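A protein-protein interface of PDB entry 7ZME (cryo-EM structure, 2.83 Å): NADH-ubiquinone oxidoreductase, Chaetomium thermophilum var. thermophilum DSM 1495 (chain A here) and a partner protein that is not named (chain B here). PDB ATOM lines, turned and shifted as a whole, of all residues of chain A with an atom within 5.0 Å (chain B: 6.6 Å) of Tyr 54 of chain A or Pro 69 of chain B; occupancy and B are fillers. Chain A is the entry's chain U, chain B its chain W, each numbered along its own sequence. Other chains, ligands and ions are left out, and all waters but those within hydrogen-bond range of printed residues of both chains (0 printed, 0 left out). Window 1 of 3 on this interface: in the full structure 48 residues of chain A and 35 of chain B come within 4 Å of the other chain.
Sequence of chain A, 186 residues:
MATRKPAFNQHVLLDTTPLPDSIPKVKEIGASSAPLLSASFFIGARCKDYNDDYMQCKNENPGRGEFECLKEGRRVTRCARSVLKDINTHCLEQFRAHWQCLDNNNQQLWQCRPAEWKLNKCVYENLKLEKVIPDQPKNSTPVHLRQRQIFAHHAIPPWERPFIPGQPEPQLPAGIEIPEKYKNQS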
ATOM      1  N   TYR A  50       6.330 -22.804  25.440  1.00  0.00           N
ATOM      2  CA  TYR A  50       7.531 -22.179  26.042  1.00  0.00           C
ATOM      3  C   TYR A  50       8.731 -23.101  25.825  1.00  0.00           C
ATOM      4  O   TYR A  50       9.821 -22.604  25.527  1.00  0.00           O
ATOM      5  CB  TYR A  50       7.248 -21.912  27.521  1.00  0.00           C
ATOM      6  CG  TYR A  50       6.041 -21.043  27.764  1.00  0.00           C
ATOM      7  CD1 TYR A  50       6.150 -19.665  27.783  1.00  0.00           C
ATOM      8  CD2 TYR A  50       4.787 -21.596  27.961  1.00  0.00           C
ATOM      9  CE1 TYR A  50       5.051 -18.855  28.004  1.00  0.00           C
ATOM     10  CE2 TYR A  50       3.676 -20.800  28.178  1.00  0.00           C
ATOM     11  CZ  TYR A  50       3.809 -19.425  28.202  1.00  0.00           C
ATOM     12  OH  TYR A  50       2.719 -18.634  28.420  1.00  0.00           O
ATOM     13  N   ASN A  51       8.521 -24.409  25.946  1.00  0.00           N
ATOM     14  CA  ASN A  51       9.603 -25.390  25.686  1.00  0.00           C
ATOM     15  C   ASN A  51      10.040 -25.241  24.232  1.00  0.00           C
ATOM     16  O   ASN A  51      11.244 -25.328  23.971  1.00  0.00           O
ATOM     17  CB  ASN A  51       9.145 -26.826  25.941  1.00  0.00           C
ATOM     18  CG  ASN A  51       9.175 -27.226  27.398  1.00  0.00           C
ATOM     19  OD1 ASN A  51       9.729 -26.514  28.233  1.00  0.00           O
ATOM     20  ND2 ASN A  51       8.587 -28.368  27.709  1.00  0.00           N
ATOM     21  N   ASP A  52       9.094 -24.988  23.332  1.00  0.00           N
ATOM     22  CA  ASP A  52       9.410 -24.879  21.886  1.00  0.00           C
ATOM     23  C   ASP A  52       9.951 -23.485  21.591  1.00  0.00           C
ATOM     24  O   ASP A  52      10.747 -23.365  20.659  1.00  0.00           O
ATOM     25  CB  ASP A  52       8.182 -25.189  21.033  1.00  0.00           C
ATOM     26  CG  ASP A  52       7.838 -26.665  20.954  1.00  0.00           C
ATOM     27  OD1 ASP A  52       8.692 -27.486  21.321  1.00  0.00           O
ATOM     28  OD2 ASP A  52       6.715 -26.978  20.521  1.00  0.00           O
ATOM     29  N   ASP A  53       9.560 -22.484  22.377  1.00  0.00           N
ATOM     30  CA  ASP A  53      10.000 -21.087  22.133  1.00  0.00           C
ATOM     31  C   ASP A  53      11.455 -20.976  22.553  1.00  0.00           C
ATOM     32  O   ASP A  53      12.232 -20.365  21.805  1.00  0.00           O
ATOM     33  CB  ASP A  53       9.198 -20.086  22.955  1.00  0.00           C
ATOM     34  CG  ASP A  53       9.389 -18.642  22.529  1.00  0.00           C
ATOM     35  OD1 ASP A  53       9.320 -18.376  21.315  1.00  0.00           O
ATOM     36  OD2 ASP A  53       9.605 -17.797  23.417  1.00  0.00           O
ATOM     37  N   TYR A  54      11.863 -21.607  23.653  1.00  0.00           N
ATOM     38  CA  TYR A  54      13.266 -21.450  24.108  1.00  0.00           C
ATOM     39  C   TYR A  54      14.205 -22.129  23.103  1.00  0.00           C
ATOM     40  O   TYR A  54      15.311 -21.608  22.889  1.00  0.00           O
ATOM     41  CB  TYR A  54      13.403 -22.066  25.501  1.00  0.00           C
ATOM     42  CG  TYR A  54      14.803 -22.256  26.021  1.00  0.00           C
ATOM     43  CD1 TYR A  54      15.603 -21.170  26.329  1.00  0.00           C
ATOM     44  CD2 TYR A  54      15.323 -23.523  26.227  1.00  0.00           C
ATOM     45  CE1 TYR A  54      16.888 -21.334  26.816  1.00  0.00           C
ATOM     46  CE2 TYR A  54      16.605 -23.706  26.712  1.00  0.00           C
ATOM     47  CZ  TYR A  54      17.388 -22.607  27.012  1.00  0.00           C
ATOM     48  OH  TYR A  54      18.653 -22.767  27.491  1.00  0.00           O
ATOM     49  N   MET A  55      13.774 -23.228  22.494  1.00  0.00           N
ATOM     50  CA  MET A  55      14.600 -23.996  21.523  1.00  0.00           C
ATOM     51  C   MET A  55      14.736 -23.248  20.198  1.00  0.00           C
ATOM     52  O   MET A  55      15.802 -23.351  19.581  1.00  0.00           O
ATOM     53  CB  MET A  55      14.028 -25.403  21.326  1.00  0.00           C
ATOM     54  CG  MET A  55      14.018 -26.228  22.594  1.00  0.00           C
ATOM     55  SD  MET A  55      15.667 -26.549  23.255  1.00  0.00           S
ATOM     56  CE  MET A  55      16.229 -27.841  22.149  1.00  0.00           C
ATOM     57  N   GLN A  56      13.681 -22.542  19.784  1.00  0.00           N
ATOM     58  CA  GLN A  56      13.689 -21.747  18.530  1.00  0.00           C
ATOM     59  C   GLN A  56      14.470 -20.461  18.796  1.00  0.00           C
ATOM     60  O   GLN A  56      15.059 -19.943  17.838  1.00  0.00           O
ATOM     61  CB  GLN A  56      12.267 -21.407  18.102  1.00  0.00           C
ATOM     62  CG  GLN A  56      11.456 -22.594  17.610  1.00  0.00           C
ATOM     63  CD  GLN A  56       9.987 -22.253  17.568  1.00  0.00           C
ATOM     64  OE1 GLN A  56       9.181 -22.964  16.974  1.00  0.00           O
ATOM     65  NE2 GLN A  56       9.627 -21.151  18.203  1.00  0.00           N
ATOM     66  N   CYS A  57      14.502 -19.981  20.044  1.00  0.00           N
ATOM     67  CA  CYS A  57      15.363 -18.842  20.340  1.00  0.00           C
ATOM     68  C   CYS A  57      16.829 -19.204  20.158  1.00  0.00           C
ATOM     69  O   CYS A  57      17.595 -18.458  19.541  1.00  0.00           O
ATOM     70  CB  CYS A  57      15.103 -18.352  21.766  1.00  0.00           C
ATOM     71  SG  CYS A  57      16.166 -17.002  22.326  1.00  0.00           S
ATOM     72  N   LYS A  58      17.239 -20.353  20.698  1.00  0.00           N
ATOM     73  CA  LYS A  58      18.638 -20.752  20.609  1.00  0.00           C
ATOM     74  C   LYS A  58      19.049 -21.004  19.168  1.00  0.00           C
ATOM     75  O   LYS A  58      20.166 -20.659  18.768  1.00  0.00           O
ATOM     76  CB  LYS A  58      18.886 -21.984  21.473  1.00  0.00           C
ATOM     77  CG  LYS A  58      18.860 -21.688  22.956  1.00  0.00           C
ATOM     78  CD  LYS A  58      18.996 -22.946  23.772  1.00  0.00           C
ATOM     79  CE  LYS A  58      20.440 -23.205  24.138  1.00  0.00           C
ATOM     80  NZ  LYS A  58      20.540 -24.272  25.168  1.00  0.00           N
ATOM     81  N   CYS A  69      19.421 -16.263  25.360  1.00  0.00           N
ATOM     82  CA  CYS A  69      18.029 -16.755  25.563  1.00  0.00           C
ATOM     83  C   CYS A  69      17.772 -17.022  27.053  1.00  0.00           C
ATOM     84  O   CYS A  69      16.994 -17.942  27.358  1.00  0.00           O
ATOM     85  CB  CYS A  69      17.747 -18.014  24.751  1.00  0.00           C
ATOM     86  SG  CYS A  69      17.926 -17.821  22.959  1.00  0.00           S
ATOM     87  N   GLU A  72      13.842 -16.676  28.122  1.00  0.00           N
ATOM     88  CA  GLU A  72      13.002 -17.805  27.663  1.00  0.00           C
ATOM     89  C   GLU A  72      13.254 -18.999  28.581  1.00  0.00           C
ATOM     90  O   GLU A  72      12.288 -19.682  28.911  1.00  0.00           O
ATOM     91  CB  GLU A  72      13.292 -18.098  26.192  1.00  0.00           C
ATOM     92  CG  GLU A  72      12.799 -17.026  25.239  1.00  0.00           C
ATOM     93  CD  GLU A  72      13.628 -15.755  25.169  1.00  0.00           C
ATOM     94  OE1 GLU A  72      14.785 -15.776  25.626  1.00  0.00           O
ATOM     95  OE2 GLU A  72      13.108 -14.745  24.660  1.00  0.00           O
ATOM     96  N   GLY A  73      14.510 -19.225  28.968  1.00  0.00           N
ATOM     97  CA  GLY A  73      14.878 -20.309  29.897  1.00  0.00           C
ATOM     98  C   GLY A  73      14.246 -20.108  31.254  1.00  0.00           C
ATOM     99  O   GLY A  73      13.780 -21.095  31.824  1.00  0.00           O
ATOM    100  N   VAL A  76      10.655 -21.159  30.963  1.00  0.00           N
ATOM    101  CA  VAL A  76      10.384 -22.628  30.901  1.00  0.00           C
ATOM    102  C   VAL A  76      10.457 -23.187  32.324  1.00  0.00           C
ATOM    103  O   VAL A  76       9.640 -24.053  32.657  1.00  0.00           O
ATOM    104  CB  VAL A  76      11.268 -23.408  29.901  1.00  0.00           C
ATOM    105  CG1 VAL A  76      11.357 -22.732  28.550  1.00  0.00           C
ATOM    106  CG2 VAL A  76      12.651 -23.732  30.437  1.00  0.00           C
ATOM    107  N   ARG B  64      11.552 -37.740  27.217  1.00  0.00           N
ATOM    108  CA  ARG B  64      12.867 -37.057  27.293  1.00  0.00           C
ATOM    109  C   ARG B  64      12.769 -35.658  26.678  1.00  0.00           C
ATOM    110  O   ARG B  64      13.306 -34.737  27.286  1.00  0.00           O
ATOM    111  CB  ARG B  64      13.979 -37.935  26.715  1.00  0.00           C
ATOM    112  CG  ARG B  64      14.396 -39.092  27.608  1.00  0.00           C
ATOM    113  CD  ARG B  64      15.612 -39.777  27.034  1.00  0.00           C
ATOM    114  NE  ARG B  64      16.084 -40.808  27.938  1.00  0.00           N
ATOM    115  CZ  ARG B  64      17.191 -41.506  27.761  1.00  0.00           C
ATOM    116  NH1 ARG B  64      17.541 -42.423  28.645  1.00  0.00           N
ATOM    117  NH2 ARG B  64      17.953 -41.276  26.709  1.00  0.00           N
ATOM    118  N   ILE B  65      12.154 -35.519  25.507  1.00  0.00           N
ATOM    119  CA  ILE B  65      12.060 -34.219  24.778  1.00  0.00           C
ATOM    120  C   ILE B  65      11.372 -33.126  25.616  1.00  0.00           C
ATOM    121  O   ILE B  65      11.861 -31.991  25.580  1.00  0.00           O
ATOM    122  CB  ILE B  65      11.336 -34.445  23.433  1.00  0.00           C
ATOM    123  CG1 ILE B  65      12.286 -34.983  22.361  1.00  0.00           C
ATOM    124  CG2 ILE B  65      10.606 -33.197  22.964  1.00  0.00           C
ATOM    125  CD1 ILE B  65      11.592 -35.769  21.279  1.00  0.00           C
ATOM    126  N   HIS B  66      10.307 -33.439  26.359  1.00  0.00           N
ATOM    127  CA  HIS B  66       9.650 -32.416  27.221  1.00  0.00           C
ATOM    128  C   HIS B  66      10.614 -31.920  28.305  1.00  0.00           C
ATOM    129  O   HIS B  66      10.524 -30.741  28.676  1.00  0.00           O
ATOM    130  CB  HIS B  66       8.311 -32.920  27.765  1.00  0.00           C
ATOM    131  CG  HIS B  66       7.353 -33.385  26.722  1.00  0.00           C
ATOM    132  ND1 HIS B  66       7.083 -32.655  25.583  1.00  0.00           N
ATOM    133  CD2 HIS B  66       6.579 -34.490  26.653  1.00  0.00           C
ATOM    134  CE1 HIS B  66       6.199 -33.299  24.850  1.00  0.00           C
ATOM    135  NE2 HIS B  66       5.874 -34.427  25.485  1.00  0.00           N
ATOM    136  N   LEU B  67      11.408 -32.814  28.878  1.00  0.00           N
ATOM    137  CA  LEU B  67      12.412 -32.459  29.917  1.00  0.00           C
ATOM    138  C   LEU B  67      13.625 -31.692  29.378  1.00  0.00           C
ATOM    139  O   LEU B  67      14.211 -30.950  30.164  1.00  0.00           O
ATOM    140  CB  LEU B  67      12.793 -33.740  30.662  1.00  0.00           C
ATOM    141  CG  LEU B  67      11.628 -34.372  31.419  1.00  0.00           C
ATOM    142  CD1 LEU B  67      12.043 -35.664  32.093  1.00  0.00           C
ATOM    143  CD2 LEU B  67      11.048 -33.397  32.432  1.00  0.00           C
ATOM    144  N   ILE B  68      13.974 -31.845  28.100  1.00  0.00           N
ATOM    145  CA  ILE B  68      15.219 -31.240  27.547  1.00  0.00           C
ATOM    146  C   ILE B  68      15.227 -29.726  27.749  1.00  0.00           C
ATOM    147  O   ILE B  68      16.274 -29.234  28.183  1.00  0.00           O
ATOM    148  CB  ILE B  68      15.407 -31.608  26.059  1.00  0.00           C
ATOM    149  CG1 ILE B  68      15.911 -33.039  25.869  1.00  0.00           C
ATOM    150  CG2 ILE B  68      16.308 -30.608  25.348  1.00  0.00           C
ATOM    151  CD1 ILE B  68      16.162 -33.406  24.428  1.00  0.00           C
ATOM    152  N   PRO B  69      14.139 -28.946  27.558  1.00  0.00           N
ATOM    153  CA  PRO B  69      14.251 -27.491  27.657  1.00  0.00           C
ATOM    154  C   PRO B  69      14.361 -26.976  29.092  1.00  0.00           C
ATOM    155  O   PRO B  69      15.007 -25.981  29.249  1.00  0.00           O
ATOM    156  CB  PRO B  69      13.000 -26.960  26.950  1.00  0.00           C
ATOM    157  CG  PRO B  69      12.512 -28.140  26.150  1.00  0.00           C
ATOM    158  CD  PRO B  69      12.821 -29.319  27.043  1.00  0.00           C
ATOM    159  N   LEU B  70      13.793 -27.670  30.087  1.00  0.00           N
ATOM    160  CA  LEU B  70      14.048 -27.205  31.476  1.00  0.00           C
ATOM    161  C   LEU B  70      15.430 -27.623  31.982  1.00  0.00           C
ATOM    162  O   LEU B  70      16.044 -26.841  32.718  1.00  0.00           O
ATOM    163  CB  LEU B  70      12.913 -27.667  32.400  1.00  0.00           C
ATOM    164  CG  LEU B  70      12.695 -29.171  32.560  1.00  0.00           C
ATOM    165  CD1 LEU B  70      13.300 -29.677  33.861  1.00  0.00           C
ATOM    166  CD2 LEU B  70      11.211 -29.494  32.528  1.00  0.00           C
ATOM    167  N   LEU B  71      15.915 -28.783  31.561  1.00  0.00           N
ATOM    168  CA  LEU B  71      17.250 -29.278  31.980  1.00  0.00           C
ATOM    169  C   LEU B  71      18.341 -28.437  31.318  1.00  0.00           C
ATOM    170  O   LEU B  71      19.255 -28.020  32.025  1.00  0.00           O
ATOM    171  CB  LEU B  71      17.352 -30.772  31.670  1.00  0.00           C
ATOM    172  CG  LEU B  71      16.534 -31.692  32.573  1.00  0.00           C
ATOM    173  CD1 LEU B  71      16.378 -33.061  31.938  1.00  0.00           C
ATOM    174  CD2 LEU B  71      17.166 -31.807  33.947  1.00  0.00           C
ATOM    175  N   GLN B  72      18.257 -28.233  30.007  1.00  0.00           N
ATOM    176  CA  GLN B  72      19.250 -27.431  29.248  1.00  0.00           C
ATOM    177  C   GLN B  72      19.243 -25.985  29.741  1.00  0.00           C
ATOM    178  O   GLN B  72      20.304 -25.366  29.716  1.00  0.00           O
ATOM    179  CB  GLN B  72      18.984 -27.546  27.748  1.00  0.00           C
ATOM    180  CG  GLN B  72      20.086 -26.967  26.875  1.00  0.00           C
ATOM    181  CD  GLN B  72      21.428 -27.628  27.069  1.00  0.00           C
ATOM    182  OE1 GLN B  72      21.526 -28.798  27.421  1.00  0.00           O
ATOM    183  NE2 GLN B  72      22.485 -26.874  26.819  1.00  0.00           N
ATOM    184  N   ALA B  73      18.105 -25.480  30.212  1.00  0.00           N
ATOM    185  CA  ALA B  73      18.011 -24.071  30.655  1.00  0.00           C
ATOM    186  C   ALA B  73      18.802 -23.909  31.953  1.00  0.00           C
ATOM    187  O   ALA B  73      19.533 -22.920  32.063  1.00  0.00           O
ATOM    188  CB  ALA B  73      16.565 -23.735  30.874  1.00  0.00           C
ATOM    189  N   GLU B  74      18.684 -24.857  32.878  1.00  0.00           N
ATOM    190  CA  GLU B  74      19.468 -24.863  34.131  1.00  0.00           C
ATOM    191  C   GLU B  74      20.949 -25.002  33.810  1.00  0.00           C
ATOM    192  O   GLU B  74      21.754 -24.359  34.500  1.00  0.00           O
ATOM    193  CB  GLU B  74      19.044 -26.095  34.914  1.00  0.00           C
ATOM    194  CG  GLU B  74      19.760 -26.266  36.238  1.00  0.00           C
ATOM    195  CD  GLU B  74      19.785 -27.701  36.725  1.00  0.00           C
ATOM    196  OE1 GLU B  74      18.972 -28.506  36.237  1.00  0.00           O
ATOM    197  OE2 GLU B  74      20.631 -28.012  37.575  1.00  0.00           O
ATOM    198  N   ASP B  76      22.505 -24.083  31.038  1.00  0.00           N
ATOM    199  CA  ASP B  76      22.972 -22.836  30.382  1.00  0.00           C
ATOM    200  C   ASP B  76      23.169 -21.745  31.425  1.00  0.00           C
ATOM    201  O   ASP B  76      24.123 -20.985  31.285  1.00  0.00           O
ATOM    202  CB  ASP B  76      21.962 -22.330  29.357  1.00  0.00           C
ATOM    203  CG  ASP B  76      21.907 -23.143  28.083  1.00  0.00           C
ATOM    204  OD1 ASP B  76      22.482 -24.244  28.056  1.00  0.00           O
ATOM    205  OD2 ASP B  76      21.296 -22.654  27.127  1.00  0.00           O
ATOM    206  N   ARG B  77      22.289 -21.681  32.425  1.00  0.00           N
ATOM    207  CA  ARG B  77      22.449 -20.671  33.500  1.00  0.00           C
ATOM    208  C   ARG B  77      23.766 -20.927  34.228  1.00  0.00           C
ATOM    209  O   ARG B  77      24.433 -19.948  34.562  1.00  0.00           O
ATOM    210  CB  ARG B  77      21.231 -20.677  34.428  1.00  0.00           C
ATOM    211  CG  ARG B  77      20.026 -19.927  33.886  1.00  0.00           C
ATOM    212  CD  ARG B  77      18.955 -19.844  34.949  1.00  0.00           C
ATOM    213  NE  ARG B  77      18.326 -21.123  35.227  1.00  0.00           N
ATOM    214  CZ  ARG B  77      17.185 -21.529  34.689  1.00  0.00           C
ATOM    215  NH1 ARG B  77      16.539 -20.749  33.842  1.00  0.00           N
ATOM    216  NH2 ARG B  77      16.692 -22.711  35.004  1.00  0.00           N
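Of the 13 printed residues of chain B, 7 touch a printed residue of chain A.
Along chain B the printed residues that touch a printed residue of chain A span positions 66 to 77.
Among the printed residues, Asp or Glu carboxylates within 4 Å of a Lys or Arg side-chain nitrogen of the other chain: Lys 58 of chain A with Asp 76 of chain B.
Tyr 54 of chain A touches four residues of chain B.
Pro 69 of chain B touches just these residues of chain A: Asn 51, Tyr 54 and Val 76.
Of the printed residues of chain A, Ala 73 of chain B touches Tyr 54 (3.5 Å), Gly 73 (3.9 Å) and Val 76 (3.9 Å).
Printed residues of chain A within 4 Å of His 66 of chain B: Asn 51.
Of the printed residues of chain A, Arg 77 of chain B touches Gly 73 (3.4 Å).
Of the printed residues of chain A, Asp 76 of chain B touches Tyr 54 (2.7 Å) and Lys 58 (2.7 Å).
Arg 64 of chain B touches none of the printed residues of chain A.
Leu 67 of chain B touches none of the printed residues of chain A.
The nearest residue of chain B that does not touch Tyr 54 of chain A is Ile 68 of chain B (5.7 Å).
The nearest residue of chain A that does not touch Pro 69 of chain B is Met 55 of chain A (4.3 Å).
The nearest printed residue of chain B that does not touch Val 76 of chain A is Arg 77 of chain B (6.0 Å).
ND2 of Asn 51 of chain A is in hydrogen-bond range of O of His 66 of chain B, 3.2 Å away.
The side-chain hydroxyl of Tyr 54 of chain A is in hydrogen-bond range of the side-chain carboxylate of Asp 76 of chain B, 2.7 Å away.
OD2 of Asp 76 of chain B lies within salt-bridge range of NZ of Lys 58 of chain A.
The guanidinium group (NH1) of Arg 77 of chain B is in hydrogen-bond range of the backbone carbonyl oxygen (O) of Gly 73 of chain A, at 3.4 Å.
OD1 of Asn 51 of chain A touches CB of Pro 69 of chain B, 3.5 Å away.
Tyr 54 of chain A touches Pro 69 of chain B (CE2 to O, 3.8 Å).
Tyr 54 of chain A touches Gln 72 of chain B (OH to O, 3.8 Å).
CA of Ala 73 of chain B touches OH of Tyr 54 of chain A, at 3.5 Å.
NZ of Lys 58 of chain A touches CG of Gln 72 of chain B (3.2 Å).
Ala 73 of chain B touches Gly 73 of chain A.
CG2 of Val 76 of chain A touches O of Pro 69 of chain B, 3.5 Å away.
CG2 of Val 76 of chain A touches CA of Leu 70 of chain B, 3.9 Å away.
Val 76 of chain A touches Ala 73 of chain B.
The side-chain amino group of Lys 58 of chain A is in hydrogen-bond range of the side-chain hydroxyl of Tyr 54 of chain A.
The backbone NH of Lys 58 of chain A lies within hydrogen-bond range of the side-chain sulfur of Cys 69 of chain A, 3.5 Å away.
The side-chain amide nitrogen (NE2) of Gln 72 of chain B is in hydrogen-bond range of the side-chain carboxylate (OD1) of Asp 76 of chain B, 2.9 Å away.
The side-chain sulfur of Cys 69 of chain A is disulfide-bonded to the side-chain sulfur of Cys 57 of chain A (2.0 Å).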
